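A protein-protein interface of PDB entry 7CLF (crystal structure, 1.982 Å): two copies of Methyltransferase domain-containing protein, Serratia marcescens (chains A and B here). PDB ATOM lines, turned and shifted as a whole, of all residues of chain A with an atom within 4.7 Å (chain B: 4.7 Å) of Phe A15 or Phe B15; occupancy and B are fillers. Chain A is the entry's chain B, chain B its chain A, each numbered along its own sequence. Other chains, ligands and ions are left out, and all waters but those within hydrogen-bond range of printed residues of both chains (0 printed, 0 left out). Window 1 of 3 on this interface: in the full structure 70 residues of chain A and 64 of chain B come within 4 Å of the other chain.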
ATOM      1  N   MET A  12      -1.039  -7.336 -16.776  1.00  0.00           N
ATOM      2  CA  MET A  12      -1.454  -6.463 -17.865  1.00  0.00           C
ATOM      3  C   MET A  12      -2.521  -7.123 -18.735  1.00  0.00           C
ATOM      4  O   MET A  12      -3.404  -6.432 -19.252  1.00  0.00           O
ATOM      5  CB  MET A  12      -0.246  -6.057 -18.713  1.00  0.00           C
ATOM      6  CG  MET A  12       0.673  -5.025 -18.039  1.00  0.00           C
ATOM      7  SD  MET A  12       2.290  -4.920 -18.834  1.00  0.00           S
ATOM      8  CE  MET A  12       1.921  -3.901 -20.267  1.00  0.00           C
ATOM      9  N   MET A  13      -2.458  -8.444 -18.903  1.00  0.00           N
ATOM     10  CA  MET A  13      -3.445  -9.203 -19.666  1.00  0.00           C
ATOM     11  C   MET A  13      -4.627  -9.660 -18.828  1.00  0.00           C
ATOM     12  O   MET A  13      -5.492 -10.375 -19.344  1.00  0.00           O
ATOM     13  CB  MET A  13      -2.803 -10.438 -20.293  1.00  0.00           C
ATOM     14  CG  MET A  13      -1.490 -10.161 -20.951  1.00  0.00           C
ATOM     15  SD  MET A  13      -1.662  -8.977 -22.286  1.00  0.00           S
ATOM     16  CE  MET A  13      -1.869 -10.136 -23.629  1.00  0.00           C
ATOM     17  N   GLY A  14      -4.690  -9.269 -17.558  1.00  0.00           N
ATOM     18  CA  GLY A  14      -5.748  -9.738 -16.676  1.00  0.00           C
ATOM     19  C   GLY A  14      -7.150  -9.318 -17.078  1.00  0.00           C
ATOM     20  O   GLY A  14      -8.124  -9.869 -16.552  1.00  0.00           O
ATOM     21  N   PHE A  15      -7.291  -8.341 -17.976  1.00  0.00           N
ATOM     22  CA  PHE A  15      -8.630  -8.058 -18.486  1.00  0.00           C
ATOM     23  C   PHE A  15      -9.172  -9.206 -19.329  1.00  0.00           C
ATOM     24  O   PHE A  15     -10.386  -9.260 -19.566  1.00  0.00           O
ATOM     25  CB  PHE A  15      -8.654  -6.746 -19.274  1.00  0.00           C
ATOM     26  CG  PHE A  15      -7.798  -6.754 -20.513  1.00  0.00           C
ATOM     27  CD1 PHE A  15      -6.426  -6.580 -20.426  1.00  0.00           C
ATOM     28  CD2 PHE A  15      -8.376  -6.907 -21.765  1.00  0.00           C
ATOM     29  CE1 PHE A  15      -5.642  -6.575 -21.576  1.00  0.00           C
ATOM     30  CE2 PHE A  15      -7.602  -6.889 -22.908  1.00  0.00           C
ATOM     31  CZ  PHE A  15      -6.235  -6.724 -22.814  1.00  0.00           C
ATOM     32  N   PHE A  16      -8.300 -10.114 -19.782  1.00  0.00           N
ATOM     33  CA  PHE A  16      -8.721 -11.354 -20.432  1.00  0.00           C
ATOM     34  C   PHE A  16      -9.646 -12.164 -19.530  1.00  0.00           C
ATOM     35  O   PHE A  16     -10.787 -12.478 -19.899  1.00  0.00           O
ATOM     36  CB  PHE A  16      -7.496 -12.203 -20.774  1.00  0.00           C
ATOM     37  CG  PHE A  16      -6.755 -11.774 -22.014  1.00  0.00           C
ATOM     38  CD1 PHE A  16      -7.056 -10.589 -22.662  1.00  0.00           C
ATOM     39  CD2 PHE A  16      -5.758 -12.587 -22.531  1.00  0.00           C
ATOM     40  CE1 PHE A  16      -6.366 -10.225 -23.827  1.00  0.00           C
ATOM     41  CE2 PHE A  16      -5.071 -12.231 -23.694  1.00  0.00           C
ATOM     42  CZ  PHE A  16      -5.376 -11.046 -24.331  1.00  0.00           C
ATOM     43  N   GLN A  17      -9.136 -12.567 -18.357  1.00  0.00           N
ATOM     44  CA  GLN A  17      -9.936 -13.347 -17.415  1.00  0.00           C
ATOM     45  C   GLN A  17     -11.164 -12.580 -16.966  1.00  0.00           C
ATOM     46  O   GLN A  17     -12.242 -13.163 -16.799  1.00  0.00           O
ATOM     47  CB  GLN A  17      -9.108 -13.727 -16.182  1.00  0.00           C
ATOM     48  CG  GLN A  17      -8.069 -14.793 -16.420  1.00  0.00           C
ATOM     49  CD  GLN A  17      -6.717 -14.214 -16.792  1.00  0.00           C
ATOM     50  OE1 GLN A  17      -6.618 -13.078 -17.260  1.00  0.00           O
ATOM     51  NE2 GLN A  17      -5.667 -14.999 -16.589  1.00  0.00           N
ATOM     52  N   ALA A  18     -11.011 -11.279 -16.731  1.00  0.00           N
ATOM     53  CA  ALA A  18     -12.120 -10.468 -16.249  1.00  0.00           C
ATOM     54  C   ALA A  18     -13.313 -10.549 -17.193  1.00  0.00           C
ATOM     55  O   ALA A  18     -14.423 -10.899 -16.784  1.00  0.00           O
ATOM     56  CB  ALA A  18     -11.665  -9.022 -16.071  1.00  0.00           C
ATOM     57  N   LYS A  19     -13.094 -10.231 -18.470  1.00  0.00           N
ATOM     58  CA  LYS A  19     -14.186 -10.230 -19.434  1.00  0.00           C
ATOM     59  C   LYS A  19     -14.679 -11.633 -19.750  1.00  0.00           C
ATOM     60  O   LYS A  19     -15.860 -11.803 -20.056  1.00  0.00           O
ATOM     61  CB  LYS A  19     -13.751  -9.517 -20.719  1.00  0.00           C
ATOM     62  CG  LYS A  19     -14.021  -8.009 -20.702  1.00  0.00           C
ATOM     63  CD  LYS A  19     -15.521  -7.705 -20.760  1.00  0.00           C
ATOM     64  CE  LYS A  19     -15.773  -6.193 -20.764  1.00  0.00           C
ATOM     65  NZ  LYS A  19     -17.211  -5.799 -21.006  1.00  0.00           N
ATOM     66  N   ILE A  99     -19.845  -3.886 -14.116  1.00  0.00           N
ATOM     67  CA  ILE A  99     -18.549  -3.841 -14.794  1.00  0.00           C
ATOM     68  C   ILE A  99     -18.720  -3.584 -16.291  1.00  0.00           C
ATOM     69  O   ILE A  99     -18.031  -2.738 -16.874  1.00  0.00           O
ATOM     70  CB  ILE A  99     -17.766  -5.142 -14.545  1.00  0.00           C
ATOM     71  CG1 ILE A  99     -17.253  -5.176 -13.099  1.00  0.00           C
ATOM     72  CG2 ILE A  99     -16.598  -5.248 -15.544  1.00  0.00           C
ATOM     73  CD1 ILE A  99     -16.746  -6.515 -12.670  1.00  0.00           C
ATOM     74  N   LEU A 103     -17.914   0.315 -15.272  1.00  0.00           N
ATOM     75  CA  LEU A 103     -16.551   0.352 -14.750  1.00  0.00           C
ATOM     76  C   LEU A 103     -15.527   0.058 -15.838  1.00  0.00           C
ATOM     77  O   LEU A 103     -14.501   0.735 -15.931  1.00  0.00           O
ATOM     78  CB  LEU A 103     -16.402  -0.628 -13.588  1.00  0.00           C
ATOM     79  CG  LEU A 103     -17.285  -0.235 -12.394  1.00  0.00           C
ATOM     80  CD1 LEU A 103     -16.899  -0.995 -11.141  1.00  0.00           C
ATOM     81  CD2 LEU A 103     -17.216   1.267 -12.154  1.00  0.00           C
ATOM     82  N   TYR A 104     -15.760  -0.976 -16.636  1.00  0.00           N
ATOM     83  CA  TYR A 104     -14.775  -1.329 -17.656  1.00  0.00           C
ATOM     84  C   TYR A 104     -14.567  -0.199 -18.651  1.00  0.00           C
ATOM     85  O   TYR A 104     -13.401   0.152 -18.912  1.00  0.00           O
ATOM     86  CB  TYR A 104     -15.176  -2.644 -18.337  1.00  0.00           C
ATOM     87  CG  TYR A 104     -14.131  -3.254 -19.250  1.00  0.00           C
ATOM     88  CD1 TYR A 104     -14.007  -2.837 -20.563  1.00  0.00           C
ATOM     89  CD2 TYR A 104     -13.297  -4.277 -18.806  1.00  0.00           C
ATOM     90  CE1 TYR A 104     -13.076  -3.403 -21.411  1.00  0.00           C
ATOM     91  CE2 TYR A 104     -12.368  -4.853 -19.642  1.00  0.00           C
ATOM     92  CZ  TYR A 104     -12.255  -4.400 -20.948  1.00  0.00           C
ATOM     93  OH  TYR A 104     -11.335  -4.952 -21.803  1.00  0.00           O
ATOM     94  N   TRP A 107     -12.588   2.775 -16.834  1.00  0.00           N
ATOM     95  CA  TRP A 107     -11.180   2.463 -16.615  1.00  0.00           C
ATOM     96  C   TRP A 107     -10.389   2.503 -17.911  1.00  0.00           C
ATOM     97  O   TRP A 107      -9.155   2.590 -17.873  1.00  0.00           O
ATOM     98  CB  TRP A 107     -11.028   1.089 -15.965  1.00  0.00           C
ATOM     99  CG  TRP A 107     -11.187   1.089 -14.468  1.00  0.00           C
ATOM    100  CD1 TRP A 107     -12.345   1.156 -13.774  1.00  0.00           C
ATOM    101  CD2 TRP A 107     -10.137   1.004 -13.491  1.00  0.00           C
ATOM    102  NE1 TRP A 107     -12.095   1.119 -12.414  1.00  0.00           N
ATOM    103  CE2 TRP A 107     -10.746   1.024 -12.217  1.00  0.00           C
ATOM    104  CE3 TRP A 107      -8.748   0.920 -13.569  1.00  0.00           C
ATOM    105  CZ2 TRP A 107     -10.016   0.965 -11.042  1.00  0.00           C
ATOM    106  CZ3 TRP A 107      -8.018   0.850 -12.397  1.00  0.00           C
ATOM    107  CH2 TRP A 107      -8.652   0.874 -11.152  1.00  0.00           C
ATOM    108  N   MET B  12     -12.758 -11.073 -11.827  1.00  0.00           N
ATOM    109  CA  MET B  12     -13.710 -10.211 -12.519  1.00  0.00           C
ATOM    110  C   MET B  12     -13.264  -8.759 -12.515  1.00  0.00           C
ATOM    111  O   MET B  12     -13.586  -8.012 -13.443  1.00  0.00           O
ATOM    112  CB  MET B  12     -15.103 -10.335 -11.894  1.00  0.00           C
ATOM    113  CG  MET B  12     -15.840 -11.581 -12.325  1.00  0.00           C
ATOM    114  SD  MET B  12     -17.425 -11.720 -11.480  1.00  0.00           S
ATOM    115  CE  MET B  12     -18.285 -10.277 -12.068  1.00  0.00           C
ATOM    116  N   MET B  13     -12.538  -8.338 -11.483  1.00  0.00           N
ATOM    117  CA  MET B  13     -12.050  -6.972 -11.377  1.00  0.00           C
ATOM    118  C   MET B  13     -10.565  -6.853 -11.736  1.00  0.00           C
ATOM    119  O   MET B  13      -9.942  -5.824 -11.451  1.00  0.00           O
ATOM    120  CB  MET B  13     -12.343  -6.449  -9.963  1.00  0.00           C
ATOM    121  CG  MET B  13     -13.854  -6.462  -9.669  1.00  0.00           C
ATOM    122  SD  MET B  13     -14.274  -5.974  -8.002  1.00  0.00           S
ATOM    123  CE  MET B  13     -14.673  -4.258  -8.280  1.00  0.00           C
ATOM    124  N   GLY B  14      -9.997  -7.884 -12.366  1.00  0.00           N
ATOM    125  CA  GLY B  14      -8.610  -7.895 -12.806  1.00  0.00           C
ATOM    126  C   GLY B  14      -8.267  -6.847 -13.847  1.00  0.00           C
ATOM    127  O   GLY B  14      -7.075  -6.626 -14.101  1.00  0.00           O
ATOM    128  N   PHE B  15      -9.270  -6.205 -14.461  1.00  0.00           N
ATOM    129  CA  PHE B  15      -8.981  -5.063 -15.327  1.00  0.00           C
ATOM    130  C   PHE B  15      -8.515  -3.846 -14.525  1.00  0.00           C
ATOM    131  O   PHE B  15      -7.895  -2.943 -15.106  1.00  0.00           O
ATOM    132  CB  PHE B  15     -10.210  -4.732 -16.214  1.00  0.00           C
ATOM    133  CG  PHE B  15     -11.416  -4.213 -15.447  1.00  0.00           C
ATOM    134  CD1 PHE B  15     -12.285  -5.093 -14.807  1.00  0.00           C
ATOM    135  CD2 PHE B  15     -11.674  -2.853 -15.365  1.00  0.00           C
ATOM    136  CE1 PHE B  15     -13.399  -4.633 -14.100  1.00  0.00           C
ATOM    137  CE2 PHE B  15     -12.777  -2.380 -14.650  1.00  0.00           C
ATOM    138  CZ  PHE B  15     -13.646  -3.278 -14.023  1.00  0.00           C
ATOM    139  N   PHE B  16      -8.756  -3.817 -13.199  1.00  0.00           N
ATOM    140  CA  PHE B  16      -8.221  -2.748 -12.362  1.00  0.00           C
ATOM    141  C   PHE B  16      -6.696  -2.736 -12.417  1.00  0.00           C
ATOM    142  O   PHE B  16      -6.072  -1.711 -12.716  1.00  0.00           O
ATOM    143  CB  PHE B  16      -8.659  -2.917 -10.901  1.00  0.00           C
ATOM    144  CG  PHE B  16     -10.098  -2.575 -10.615  1.00  0.00           C
ATOM    145  CD1 PHE B  16     -11.011  -2.288 -11.627  1.00  0.00           C
ATOM    146  CD2 PHE B  16     -10.546  -2.555  -9.292  1.00  0.00           C
ATOM    147  CE1 PHE B  16     -12.331  -1.981 -11.315  1.00  0.00           C
ATOM    148  CE2 PHE B  16     -11.854  -2.250  -8.984  1.00  0.00           C
ATOM    149  CZ  PHE B  16     -12.750  -1.968  -9.991  1.00  0.00           C
ATOM    150  N   GLN B  17      -6.083  -3.875 -12.089  1.00  0.00           N
ATOM    151  CA  GLN B  17      -4.627  -3.992 -12.118  1.00  0.00           C
ATOM    152  C   GLN B  17      -4.092  -3.718 -13.514  1.00  0.00           C
ATOM    153  O   GLN B  17      -3.067  -3.041 -13.677  1.00  0.00           O
ATOM    154  CB  GLN B  17      -4.210  -5.392 -11.663  1.00  0.00           C
ATOM    155  CG  GLN B  17      -4.290  -5.634 -10.162  1.00  0.00           C
ATOM    156  CD  GLN B  17      -5.664  -6.122  -9.702  1.00  0.00           C
ATOM    157  OE1 GLN B  17      -6.662  -5.984 -10.414  1.00  0.00           O
ATOM    158  NE2 GLN B  17      -5.716  -6.691  -8.502  1.00  0.00           N
ATOM    159  N   ALA B  18      -4.789  -4.223 -14.536  1.00  0.00           N
ATOM    160  CA  ALA B  18      -4.274  -4.137 -15.898  1.00  0.00           C
ATOM    161  C   ALA B  18      -4.132  -2.685 -16.336  1.00  0.00           C
ATOM    162  O   ALA B  18      -3.094  -2.290 -16.874  1.00  0.00           O
ATOM    163  CB  ALA B  18      -5.181  -4.914 -16.849  1.00  0.00           C
ATOM    164  N   LYS B  19      -5.160  -1.870 -16.095  1.00  0.00           N
ATOM    165  CA  LYS B  19      -5.078  -0.461 -16.470  1.00  0.00           C
ATOM    166  C   LYS B  19      -4.196   0.345 -15.521  1.00  0.00           C
ATOM    167  O   LYS B  19      -3.629   1.365 -15.925  1.00  0.00           O
ATOM    168  CB  LYS B  19      -6.483   0.140 -16.538  1.00  0.00           C
ATOM    169  CG  LYS B  19      -7.208  -0.142 -17.890  1.00  0.00           C
ATOM    170  CD  LYS B  19      -6.595   0.697 -19.037  1.00  0.00           C
ATOM    171  CE  LYS B  19      -7.218   0.369 -20.400  1.00  0.00           C
ATOM    172  NZ  LYS B  19      -6.776   1.339 -21.457  1.00  0.00           N
ATOM    173  N   ILE B  99      -2.330  -2.853 -25.851  1.00  0.00           N
ATOM    174  CA  ILE B  99      -3.499  -3.116 -25.025  1.00  0.00           C
ATOM    175  C   ILE B  99      -4.410  -1.898 -24.990  1.00  0.00           C
ATOM    176  O   ILE B  99      -5.631  -2.009 -25.146  1.00  0.00           O
ATOM    177  CB  ILE B  99      -3.065  -3.524 -23.605  1.00  0.00           C
ATOM    178  CG1 ILE B  99      -2.501  -4.943 -23.577  1.00  0.00           C
ATOM    179  CG2 ILE B  99      -4.238  -3.386 -22.636  1.00  0.00           C
ATOM    180  CD1 ILE B  99      -1.630  -5.197 -22.318  1.00  0.00           C
ATOM    181  N   LEU B 103      -6.504  -3.946 -27.767  1.00  0.00           N
ATOM    182  CA  LEU B 103      -7.064  -5.132 -27.123  1.00  0.00           C
ATOM    183  C   LEU B 103      -8.081  -4.805 -26.030  1.00  0.00           C
ATOM    184  O   LEU B 103      -9.095  -5.494 -25.920  1.00  0.00           O
ATOM    185  CB  LEU B 103      -5.950  -5.999 -26.552  1.00  0.00           C
ATOM    186  CG  LEU B 103      -4.983  -6.591 -27.585  1.00  0.00           C
ATOM    187  CD1 LEU B 103      -4.150  -7.691 -26.930  1.00  0.00           C
ATOM    188  CD2 LEU B 103      -5.705  -7.116 -28.845  1.00  0.00           C
ATOM    189  N   TYR B 104      -7.823  -3.799 -25.188  1.00  0.00           N
ATOM    190  CA  TYR B 104      -8.780  -3.515 -24.114  1.00  0.00           C
ATOM    191  C   TYR B 104     -10.106  -3.018 -24.685  1.00  0.00           C
ATOM    192  O   TYR B 104     -11.162  -3.494 -24.240  1.00  0.00           O
ATOM    193  CB  TYR B 104      -8.169  -2.538 -23.099  1.00  0.00           C
ATOM    194  CG  TYR B 104      -8.996  -2.252 -21.848  1.00  0.00           C
ATOM    195  CD1 TYR B 104     -10.048  -1.344 -21.884  1.00  0.00           C
ATOM    196  CD2 TYR B 104      -8.694  -2.861 -20.621  1.00  0.00           C
ATOM    197  CE1 TYR B 104     -10.801  -1.062 -20.755  1.00  0.00           C
ATOM    198  CE2 TYR B 104      -9.453  -2.580 -19.463  1.00  0.00           C
ATOM    199  CZ  TYR B 104     -10.494  -1.677 -19.548  1.00  0.00           C
ATOM    200  OH  TYR B 104     -11.263  -1.371 -18.446  1.00  0.00           O
ATOM    201  N   TRP B 107     -11.872  -6.328 -26.314  1.00  0.00           N
ATOM    202  CA  TRP B 107     -12.384  -7.228 -25.276  1.00  0.00           C
ATOM    203  C   TRP B 107     -13.588  -6.647 -24.548  1.00  0.00           C
ATOM    204  O   TRP B 107     -14.351  -7.406 -23.942  1.00  0.00           O
ATOM    205  CB  TRP B 107     -11.288  -7.580 -24.251  1.00  0.00           C
ATOM    206  CG  TRP B 107     -10.398  -8.734 -24.664  1.00  0.00           C
ATOM    207  CD1 TRP B 107      -9.374  -8.699 -25.582  1.00  0.00           C
ATOM    208  CD2 TRP B 107     -10.449 -10.081 -24.181  1.00  0.00           C
ATOM    209  NE1 TRP B 107      -8.798  -9.936 -25.691  1.00  0.00           N
ATOM    210  CE2 TRP B 107      -9.441 -10.803 -24.847  1.00  0.00           C
ATOM    211  CE3 TRP B 107     -11.250 -10.748 -23.253  1.00  0.00           C
ATOM    212  CZ2 TRP B 107      -9.207 -12.158 -24.601  1.00  0.00           C
ATOM    213  CZ3 TRP B 107     -11.016 -12.095 -23.017  1.00  0.00           C
ATOM    214  CH2 TRP B 107     -10.003 -12.780 -23.684  1.00  0.00           C
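The side-chain hydroxyl (OH) of Tyr B104 is in hydrogen-bond range of the backbone carbonyl oxygen (O) of Tyr A104 (2.7 Å).
The backbone NH (N) of Tyr B104 sits at hydrogen-bond distance from the backbone carbonyl oxygen (O) of Ile B99 (2.8 Å).
The backbone NH of Tyr A104 is in hydrogen-bond range of the backbone carbonyl oxygen of Ile A99 (2.9 Å).
Among the printed residues, pairs that only touch across the chains: Met A12 with Ala B18 (3.4 Å), Met A12 with Ile B99 (3.8 Å), Met A13 with Ile B99 (3.8 Å), Phe A15 with Phe B15 (3.98 Å), Phe A15 with Ile B99 (3.6 Å), Phe A15 with Leu B103 (3.6 Å), Phe A15 with Tyr B104 (3.8 Å), Phe A15 with Trp B107 (3.7 Å), Phe A16 with Trp B107 (3.1 Å), Ala A18 with Met B12 (3.4 Å), Lys A19 with Trp B107 (3.3 Å), Ile A99 with Met B12 (3.6 Å), Ile A99 with Phe B15 (3.6 Å), Leu A103 with Phe B15 (3.8 Å), Tyr A104 with Phe B15 (3.8 Å), Tyr A104 with Trp B107 (3.6 Å), Trp A107 with Phe B15 (3.7 Å), Trp A107 with Phe B16 (3.2 Å), Trp A107 with Lys B19 (3.4 Å) and Trp A107 with Tyr B104 (3.5 Å).
Of the printed residues of chain B, Phe A15 touches Phe B15, Ile B99, Leu B103, Tyr B104 and Trp B107.
Of the printed residues of chain A, Phe B15 touches Phe A15, Ile A99, Leu A103, Tyr A104 and Trp A107.
Printed residues of chain A within 4 Å of Ala B18: Met A12 (3.4 Å).
Printed residues of chain A within 4 Å of Lys B19: Trp A107.
Of the printed residues of chain A, Trp B107 touches Phe A15, Phe A16, Lys A19 and Tyr A104.
Hydrophobic or aromatic side chains of chain A that line the printed part of chain B: Met A12, Met A13, Phe A15, Phe A16, Ala A18, Ile A99, Leu A103, Tyr A104 and Trp A107.
Printed residues of chain B that touch a printed residue of chain A: Met B12, Phe B15, Phe B16, Ala B18, Lys B19, Ile B99, Leu B103, Tyr B104 and Trp B107.
Hydrophobic or aromatic side chains of chain B within 4 Å of the printed part of chain A: Phe B15, Phe B16, Ala B18, Ile B99, Leu B103, Tyr B104 and Trp B107.
Among the printed residues, 21 pairs touch across the chains.
Met A12 touches Ile B99, and with the chains exchanged Ile A99 touches Met B12.
Met A13 touches Ile B99, but with the chains exchanged Ile A99 does not touch Met B13 (4.2 Å).
Phe A15 touches Ile B99, and with the chains exchanged Ile A99 touches Phe B15.
Tyr B104 touches its own counterpart, Tyr A104.
Of the 21 pairs that touch across the chains among the printed residues, 20 have their exchanged pair printed and touching as well.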
